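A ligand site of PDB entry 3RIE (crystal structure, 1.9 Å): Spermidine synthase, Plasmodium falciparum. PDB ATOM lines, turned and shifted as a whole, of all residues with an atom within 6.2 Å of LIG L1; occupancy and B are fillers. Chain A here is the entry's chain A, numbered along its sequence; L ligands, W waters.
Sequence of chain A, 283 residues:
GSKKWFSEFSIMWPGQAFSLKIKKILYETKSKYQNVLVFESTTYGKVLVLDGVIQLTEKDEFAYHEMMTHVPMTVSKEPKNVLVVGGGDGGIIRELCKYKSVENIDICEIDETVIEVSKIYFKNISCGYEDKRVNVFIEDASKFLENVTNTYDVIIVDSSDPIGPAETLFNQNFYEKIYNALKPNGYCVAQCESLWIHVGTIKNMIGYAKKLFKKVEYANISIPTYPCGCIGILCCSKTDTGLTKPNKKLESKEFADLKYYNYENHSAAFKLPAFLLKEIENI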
ATOM      1  N   GLU A   8      27.197  28.143  25.795  1.00  0.00           N
ATOM      2  CA  GLU A   8      26.613  28.021  24.444  1.00  0.00           C
ATOM      3  C   GLU A   8      25.142  28.508  24.436  1.00  0.00           C
ATOM      4  O   GLU A   8      24.265  27.779  24.856  1.00  0.00           O
ATOM      5  CB  GLU A   8      26.711  26.560  23.946  1.00  0.00           C
ATOM      6  CG  GLU A   8      26.275  26.364  22.494  1.00  0.00           C
ATOM      7  CD  GLU A   8      26.121  24.868  22.152  1.00  0.00           C
ATOM      8  OE1 GLU A   8      25.332  24.153  22.841  1.00  0.00           O
ATOM      9  OE2 GLU A   8      26.788  24.409  21.186  1.00  0.00           O
ATOM     10  N   TRP A  13      18.086  27.557  20.025  1.00  0.00           N
ATOM     11  CA  TRP A  13      17.487  26.843  21.155  1.00  0.00           C
ATOM     12  C   TRP A  13      17.270  27.853  22.308  1.00  0.00           C
ATOM     13  O   TRP A  13      18.027  27.840  23.276  1.00  0.00           O
ATOM     14  CB  TRP A  13      18.364  25.673  21.637  1.00  0.00           C
ATOM     15  CG  TRP A  13      19.922  25.910  21.535  1.00  0.00           C
ATOM     16  CD1 TRP A  13      20.723  26.423  22.484  1.00  0.00           C
ATOM     17  CD2 TRP A  13      20.779  25.675  20.382  1.00  0.00           C
ATOM     18  NE1 TRP A  13      22.049  26.472  22.057  1.00  0.00           N
ATOM     19  CE2 TRP A  13      22.113  25.990  20.771  1.00  0.00           C
ATOM     20  CE3 TRP A  13      20.561  25.140  19.106  1.00  0.00           C
ATOM     21  CZ2 TRP A  13      23.218  25.906  19.889  1.00  0.00           C
ATOM     22  CZ3 TRP A  13      21.692  25.033  18.210  1.00  0.00           C
ATOM     23  CH2 TRP A  13      22.993  25.389  18.628  1.00  0.00           C
ATOM     24  N   VAL A  53      29.056  28.258  18.865  1.00  0.00           N
ATOM     25  CA  VAL A  53      28.396  26.935  18.970  1.00  0.00           C
ATOM     26  C   VAL A  53      29.448  25.836  18.984  1.00  0.00           C
ATOM     27  O   VAL A  53      30.379  25.811  18.126  1.00  0.00           O
ATOM     28  CB  VAL A  53      27.430  26.696  17.756  1.00  0.00           C
ATOM     29  CG1 VAL A  53      26.844  25.255  17.726  1.00  0.00           C
ATOM     30  CG2 VAL A  53      26.323  27.724  17.757  1.00  0.00           C
ATOM     31  N   ILE A  54      29.290  24.893  19.882  1.00  0.00           N
ATOM     32  CA  ILE A  54      30.252  23.844  20.069  1.00  0.00           C
ATOM     33  C   ILE A  54      30.230  22.928  18.872  1.00  0.00           C
ATOM     34  O   ILE A  54      29.143  22.379  18.531  1.00  0.00           O
ATOM     35  CB  ILE A  54      29.941  23.041  21.378  1.00  0.00           C
ATOM     36  CG1 ILE A  54      30.157  23.941  22.594  1.00  0.00           C
ATOM     37  CG2 ILE A  54      30.870  21.861  21.496  1.00  0.00           C
ATOM     38  CD1 ILE A  54      29.590  23.326  23.989  1.00  0.00           C
ATOM     39  N   GLN A  55      31.398  22.711  18.251  1.00  0.00           N
ATOM     40  CA  GLN A  55      31.476  21.761  17.097  1.00  0.00           C
ATOM     41  C   GLN A  55      31.946  20.387  17.600  1.00  0.00           C
ATOM     42  O   GLN A  55      31.459  19.367  17.172  1.00  0.00           O
ATOM     43  CB  GLN A  55      32.441  22.276  15.992  1.00  0.00           C
ATOM     44  CG  GLN A  55      32.094  23.622  15.529  1.00  0.00           C
ATOM     45  CD  GLN A  55      30.761  23.684  14.823  1.00  0.00           C
ATOM     46  OE1 GLN A  55      30.558  22.950  13.859  1.00  0.00           O
ATOM     47  NE2 GLN A  55      29.823  24.594  15.292  1.00  0.00           N
ATOM     48  N   LEU A  56      32.895  20.359  18.511  1.00  0.00           N
ATOM     49  CA  LEU A  56      33.338  19.091  18.994  1.00  0.00           C
ATOM     50  C   LEU A  56      34.083  19.348  20.248  1.00  0.00           C
ATOM     51  O   LEU A  56      34.532  20.479  20.501  1.00  0.00           O
ATOM     52  CB  LEU A  56      34.242  18.336  17.994  1.00  0.00           C
ATOM     53  CG  LEU A  56      35.556  18.951  17.417  1.00  0.00           C
ATOM     54  CD1 LEU A  56      36.664  18.713  18.375  1.00  0.00           C
ATOM     55  CD2 LEU A  56      35.920  18.164  16.078  1.00  0.00           C
ATOM     56  N   TYR A  64      29.681  11.044  17.630  1.00  0.00           N
ATOM     57  CA  TYR A  64      29.143  11.607  16.408  1.00  0.00           C
ATOM     58  C   TYR A  64      29.926  11.158  15.122  1.00  0.00           C
ATOM     59  O   TYR A  64      29.300  10.833  14.101  1.00  0.00           O
ATOM     60  CB  TYR A  64      29.234  13.115  16.508  1.00  0.00           C
ATOM     61  CG  TYR A  64      28.802  13.880  15.300  1.00  0.00           C
ATOM     62  CD1 TYR A  64      27.477  14.063  15.026  1.00  0.00           C
ATOM     63  CD2 TYR A  64      29.777  14.453  14.439  1.00  0.00           C
ATOM     64  CE1 TYR A  64      27.050  14.796  13.862  1.00  0.00           C
ATOM     65  CE2 TYR A  64      29.389  15.167  13.343  1.00  0.00           C
ATOM     66  CZ  TYR A  64      28.033  15.356  13.074  1.00  0.00           C
ATOM     67  OH  TYR A  64      27.645  16.076  11.992  1.00  0.00           O
ATOM     68  N   HIS A  65      31.251  11.177  15.144  1.00  0.00           N
ATOM     69  CA  HIS A  65      31.977  10.861  13.896  1.00  0.00           C
ATOM     70  C   HIS A  65      31.835   9.359  13.533  1.00  0.00           C
ATOM     71  O   HIS A  65      31.641   9.045  12.379  1.00  0.00           O
ATOM     72  CB  HIS A  65      33.424  11.282  13.979  1.00  0.00           C
ATOM     73  CG  HIS A  65      33.582  12.779  14.114  1.00  0.00           C
ATOM     74  ND1 HIS A  65      34.222  13.362  15.181  1.00  0.00           N
ATOM     75  CD2 HIS A  65      33.112  13.789  13.341  1.00  0.00           C
ATOM     76  CE1 HIS A  65      34.197  14.676  15.027  1.00  0.00           C
ATOM     77  NE2 HIS A  65      33.479  14.963  13.952  1.00  0.00           N
ATOM     78  N   GLY A  87      32.818  19.366   7.686  1.00  0.00           N
ATOM     79  CA  GLY A  87      33.802  18.425   8.324  1.00  0.00           C
ATOM     80  C   GLY A  87      35.270  18.804   8.386  1.00  0.00           C
ATOM     81  O   GLY A  87      36.177  17.903   8.550  1.00  0.00           O
ATOM     82  N   GLY A  88      35.551  20.118   8.328  1.00  0.00           N
ATOM     83  CA  GLY A  88      36.930  20.633   8.343  1.00  0.00           C
ATOM     84  C   GLY A  88      37.797  20.048   9.417  1.00  0.00           C
ATOM     85  O   GLY A  88      39.006  19.933   9.250  1.00  0.00           O
ATOM     86  N   ASP A  89      37.209  19.671  10.568  1.00  0.00           N
ATOM     87  CA  ASP A  89      38.032  19.152  11.646  1.00  0.00           C
ATOM     88  C   ASP A  89      38.697  17.828  11.283  1.00  0.00           C
ATOM     89  O   ASP A  89      39.684  17.413  11.903  1.00  0.00           O
ATOM     90  CB  ASP A  89      37.167  18.954  12.940  1.00  0.00           C
ATOM     91  CG  ASP A  89      35.924  18.106  12.657  1.00  0.00           C
ATOM     92  OD1 ASP A  89      36.038  16.848  12.656  1.00  0.00           O
ATOM     93  OD2 ASP A  89      34.906  18.728  12.327  1.00  0.00           O
ATOM     94  N   GLY A  90      38.119  17.114  10.323  1.00  0.00           N
ATOM     95  CA  GLY A  90      38.674  15.829   9.839  1.00  0.00           C
ATOM     96  C   GLY A  90      38.187  14.544  10.539  1.00  0.00           C
ATOM     97  O   GLY A  90      38.604  13.440  10.188  1.00  0.00           O
ATOM     98  N   GLY A  91      37.276  14.673  11.507  1.00  0.00           N
ATOM     99  CA  GLY A  91      36.846  13.458  12.269  1.00  0.00           C
ATOM    100  C   GLY A  91      36.176  12.437  11.346  1.00  0.00           C
ATOM    101  O   GLY A  91      36.488  11.275  11.441  1.00  0.00           O
ATOM    102  N   ILE A  92      35.299  12.835  10.472  1.00  0.00           N
ATOM    103  CA  ILE A  92      34.745  11.895   9.498  1.00  0.00           C
ATOM    104  C   ILE A  92      35.810  11.264   8.629  1.00  0.00           C
ATOM    105  O   ILE A  92      35.834  10.014   8.435  1.00  0.00           O
ATOM    106  CB  ILE A  92      33.657  12.577   8.593  1.00  0.00           C
ATOM    107  CG1 ILE A  92      32.548  13.285   9.415  1.00  0.00           C
ATOM    108  CG2 ILE A  92      33.103  11.614   7.468  1.00  0.00           C
ATOM    109  CD1 ILE A  92      31.572  12.239  10.152  1.00  0.00           C
ATOM    110  N   ASP A 158      28.454  16.858   7.034  1.00  0.00           N
ATOM    111  CA  ASP A 158      28.860  17.207   8.362  1.00  0.00           C
ATOM    112  C   ASP A 158      28.991  18.728   8.433  1.00  0.00           C
ATOM    113  O   ASP A 158      30.049  19.231   8.541  1.00  0.00           O
ATOM    114  CB  ASP A 158      30.166  16.518   8.670  1.00  0.00           C
ATOM    115  CG  ASP A 158      30.693  16.801  10.046  1.00  0.00           C
ATOM    116  OD1 ASP A 158      29.966  17.204  10.922  1.00  0.00           O
ATOM    117  OD2 ASP A 158      31.854  16.601  10.230  1.00  0.00           O
ATOM    118  N   SER A 159      27.839  19.400   8.376  1.00  0.00           N
ATOM    119  CA  SER A 159      27.796  20.859   8.414  1.00  0.00           C
ATOM    120  C   SER A 159      27.661  21.378   9.861  1.00  0.00           C
ATOM    121  O   SER A 159      27.198  20.673  10.765  1.00  0.00           O
ATOM    122  CB  SER A 159      26.581  21.387   7.628  1.00  0.00           C
ATOM    123  OG  SER A 159      25.414  20.832   8.286  1.00  0.00           O
ATOM    124  N   SER A 160      28.149  22.589  10.088  1.00  0.00           N
ATOM    125  CA  SER A 160      27.704  23.431  11.199  1.00  0.00           C
ATOM    126  C   SER A 160      26.167  23.811  11.014  1.00  0.00           C
ATOM    127  O   SER A 160      25.512  23.403  10.020  1.00  0.00           O
ATOM    128  CB  SER A 160      28.578  24.688  11.241  1.00  0.00           C
ATOM    129  OG  SER A 160      28.553  25.349   9.972  1.00  0.00           O
ATOM    130  N   ASP A 161      25.621  24.601  11.949  1.00  0.00           N
ATOM    131  CA  ASP A 161      24.177  24.949  11.960  1.00  0.00           C
ATOM    132  C   ASP A 161      23.714  25.978  10.911  1.00  0.00           C
ATOM    133  O   ASP A 161      24.546  26.681  10.272  1.00  0.00           O
ATOM    134  CB  ASP A 161      23.799  25.434  13.401  1.00  0.00           C
ATOM    135  CG  ASP A 161      23.888  24.351  14.416  1.00  0.00           C
ATOM    136  OD1 ASP A 161      23.234  23.307  14.168  1.00  0.00           O
ATOM    137  OD2 ASP A 161      24.565  24.515  15.465  1.00  0.00           O
ATOM    138  N   GLN A 191      23.816  15.551   9.217  1.00  0.00           N
ATOM    139  CA  GLN A 191      23.392  15.940  10.600  1.00  0.00           C
ATOM    140  C   GLN A 191      22.078  16.764  10.550  1.00  0.00           C
ATOM    141  O   GLN A 191      21.842  17.595   9.634  1.00  0.00           O
ATOM    142  CB  GLN A 191      24.491  16.650  11.356  1.00  0.00           C
ATOM    143  CG  GLN A 191      24.805  18.071  10.962  1.00  0.00           C
ATOM    144  CD  GLN A 191      23.897  19.136  11.595  1.00  0.00           C
ATOM    145  OE1 GLN A 191      23.076  18.859  12.486  1.00  0.00           O
ATOM    146  NE2 GLN A 191      24.005  20.363  11.078  1.00  0.00           N
ATOM    147  N   TYR A 226      26.315  18.443  22.449  1.00  0.00           N
ATOM    148  CA  TYR A 226      25.387  19.118  21.514  1.00  0.00           C
ATOM    149  C   TYR A 226      24.067  19.440  22.270  1.00  0.00           C
ATOM    150  O   TYR A 226      23.725  18.740  23.238  1.00  0.00           O
ATOM    151  CB  TYR A 226      25.069  18.283  20.265  1.00  0.00           C
ATOM    152  CG  TYR A 226      26.211  18.138  19.270  1.00  0.00           C
ATOM    153  CD1 TYR A 226      27.296  19.039  19.250  1.00  0.00           C
ATOM    154  CD2 TYR A 226      26.250  17.047  18.405  1.00  0.00           C
ATOM    155  CE1 TYR A 226      28.381  18.901  18.299  1.00  0.00           C
ATOM    156  CE2 TYR A 226      27.287  16.926  17.470  1.00  0.00           C
ATOM    157  CZ  TYR A 226      28.350  17.847  17.419  1.00  0.00           C
ATOM    158  OH  TYR A 226      29.377  17.663  16.480  1.00  0.00           O
ATOM    159  N   PRO A 227      23.373  20.483  21.861  1.00  0.00           N
ATOM    160  CA  PRO A 227      22.275  20.950  22.737  1.00  0.00           C
ATOM    161  C   PRO A 227      21.182  19.886  22.824  1.00  0.00           C
ATOM    162  O   PRO A 227      20.874  19.235  21.812  1.00  0.00           O
ATOM    163  CB  PRO A 227      21.680  22.140  21.990  1.00  0.00           C
ATOM    164  CG  PRO A 227      22.531  22.349  20.752  1.00  0.00           C
ATOM    165  CD  PRO A 227      23.655  21.395  20.729  1.00  0.00           C
ATOM    166  N   ILE A 231      21.627  14.364  18.732  1.00  0.00           N
ATOM    167  CA  ILE A 231      21.543  14.913  17.395  1.00  0.00           C
ATOM    168  C   ILE A 231      21.069  13.846  16.381  1.00  0.00           C
ATOM    169  O   ILE A 231      21.443  12.678  16.479  1.00  0.00           O
ATOM    170  CB  ILE A 231      22.905  15.556  16.928  1.00  0.00           C
ATOM    171  CG1 ILE A 231      22.639  16.369  15.691  1.00  0.00           C
ATOM    172  CG2 ILE A 231      24.045  14.498  16.672  1.00  0.00           C
ATOM    173  CD1 ILE A 231      23.721  17.261  15.415  1.00  0.00           C
HETATM  174  C1  LIG L   1      31.975  18.077  14.110  1.00  0.00           C
HETATM  175  N1  LIG L   1      32.611  17.481  12.865  1.00  0.00           N
HETATM  176  C2  LIG L   1      31.040  19.217  13.679  1.00  0.00           C
HETATM  177  N2  LIG L   1      28.678  19.577  13.100  1.00  0.00           N
HETATM  178  C3  LIG L   1      29.595  18.730  13.845  1.00  0.00           C
HETATM  179  N3  LIG L   1      25.067  22.066  17.049  1.00  0.00           N
HETATM  180  C4  LIG L   1      27.660  20.265  13.990  1.00  0.00           C
HETATM  181  C5  LIG L   1      28.256  21.178  15.074  1.00  0.00           C
HETATM  182  C6  LIG L   1      27.125  22.076  15.611  1.00  0.00           C
HETATM  183  C7  LIG L   1      26.110  21.214  16.387  1.00  0.00           C
HETATM  184  C8  LIG L   1      25.505  20.166  15.459  1.00  0.00           C
HETATM  185  C9  LIG L   1      26.550  19.378  14.602  1.00  0.00           C
HETATM  186  C1  LG2 L   2      33.594  21.778  12.134  1.00  0.00           C
HETATM  187  S1  LG2 L   2      32.732  20.681  11.015  1.00  0.00           S
HETATM  188  C2  LG2 L   2      31.469  21.680  10.210  1.00  0.00           C
HETATM  189  C3  LG2 L   2      32.108  22.496   9.106  1.00  0.00           C
HETATM  190  O1  LG2 L   2      31.062  22.859   8.233  1.00  0.00           O
HETATM  191  C4  LG2 L   2      32.123  24.834   8.549  1.00  0.00           C
HETATM  192  O2  LG2 L   2      32.991  25.858   8.030  1.00  0.00           O
HETATM  193  C5  LG2 L   2      32.667  23.847   9.557  1.00  0.00           C
HETATM  194  O3  LG2 L   2      34.056  23.703   9.577  1.00  0.00           O
HETATM  195  C6  LG2 L   2      31.718  23.858   7.466  1.00  0.00           C
HETATM  196  N1  LG2 L   2      30.756  24.482   6.592  1.00  0.00           N
HETATM  197  C7  LG2 L   2      29.767  25.322   6.945  1.00  0.00           C
HETATM  198  N2  LG2 L   2      29.088  25.798   5.875  1.00  0.00           N
HETATM  199  C8  LG2 L   2      29.622  25.118   4.803  1.00  0.00           C
HETATM  200  C9  LG2 L   2      29.402  25.107   3.363  1.00  0.00           C
HETATM  201  N3  LG2 L   2      28.416  25.891   2.851  1.00  0.00           N
HETATM  202  N4  LG2 L   2      30.231  24.343   2.606  1.00  0.00           N
HETATM  203  C10 LG2 L   2      31.257  23.638   3.092  1.00  0.00           C
HETATM  204  N5  LG2 L   2      31.500  23.579   4.423  1.00  0.00           N
HETATM  205  C11 LG2 L   2      30.736  24.284   5.273  1.00  0.00           C
HETATM  206  O   HOH W   1      26.409  22.322  19.392  1.00  0.00           O
HETATM  207  O   HOH W   2      34.467  15.671  10.545  1.00  0.00           O
HETATM  208  O   HOH W   3      27.104  25.186  14.176  1.00  0.00           O
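OD2 of Asp 89 lies within salt-bridge range of N1 of LIG L1, at 2.7 Å.
NE2 of His 65 is in hydrogen-bond range of N1 of LIG L1 (2.9 Å).
The side-chain carboxylate (OD2) of Asp 158 is in salt-bridge range of a nitrogen (N1) of LIG L1.
OD2 of Asp 161 lies within salt-bridge range of N3 of LIG L1 (3.0 Å).
The backbone carbonyl oxygen (O) of Ser 159 is in hydrogen-bond range of a nitrogen (N2) of LIG L1, at 3.0 Å.
O1 of LG2 L2 sits close to N of Ser 160.
N of Gly 87 lies close to S1 of LG2 L2, 3.6 Å away.
S1 of LG2 L2 lies close to N1 of LIG L1, 3.7 Å away.
The side-chain carboxylate (OD1) of Asp 89 sits at hydrogen-bond distance from a ring nitrogen (NE2) of His 65.
N of Gly 91 lies within hydrogen-bond range of OD1 of Asp 89 (2.8 Å).
OH of Tyr 226 sits at hydrogen-bond distance from O of Gln 55, 2.8 Å away.
OD1 of Asp 158 sits at hydrogen-bond distance from OH of Tyr 64 (2.8 Å).
O of Asp 158 sits at hydrogen-bond distance from N of Gly 87.
The side-chain hydroxyl of Ser 159 sits at hydrogen-bond distance from the side-chain amide nitrogen of Gln 191 (3.2 Å).
The backbone carbonyl oxygen (O) of Val 53 is in hydrogen-bond range of the side-chain amide nitrogen (NE2) of Gln 55.
The backbone NH of Ile 54 sits at hydrogen-bond distance from the side-chain carboxylate of Glu 8, at 2.9 Å.
Val 53 touches LIG L1 (CG1 to N3, 3.7 Å).
Ile 54 touches LIG L1 (O to C6, 3.6 Å).
Gln 55 touches LIG L1.
Tyr 64 touches LIG L1 (CE2 to C3, 3.6 Å).
Tyr 226 touches LIG L1.
CD of Pro 227 touches N3 of LIG L1, 3.998 Å away.
CD1 of Ile 231 touches C8 of LIG L1, at 3.4 Å.
Hydrophobic or aromatic side chains within 4 Å of LIG L1: Val 53, Tyr 64, His 65, Tyr 226, Pro 227 and Ile 231.
Within 4 Å of LIG L1: Val 53, Ile 54, Gln 55, Tyr 64, His 65, Asp 89, Asp 158, Ser 159, Asp 161, Tyr 226, Pro 227 and Ile 231.
Water W1 lies within hydrogen-bond range of a nitrogen (N3) of LIG L1 (2.7 Å), the side-chain carboxylate of Glu 8 (2.8 Å) and the backbone carbonyl oxygen of Ile 54 (2.9 Å).
Water W3 bridges the backbone NH of Asp 161 (2.7 Å) and the side-chain amide nitrogen of Gln 55 (3.0 Å).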
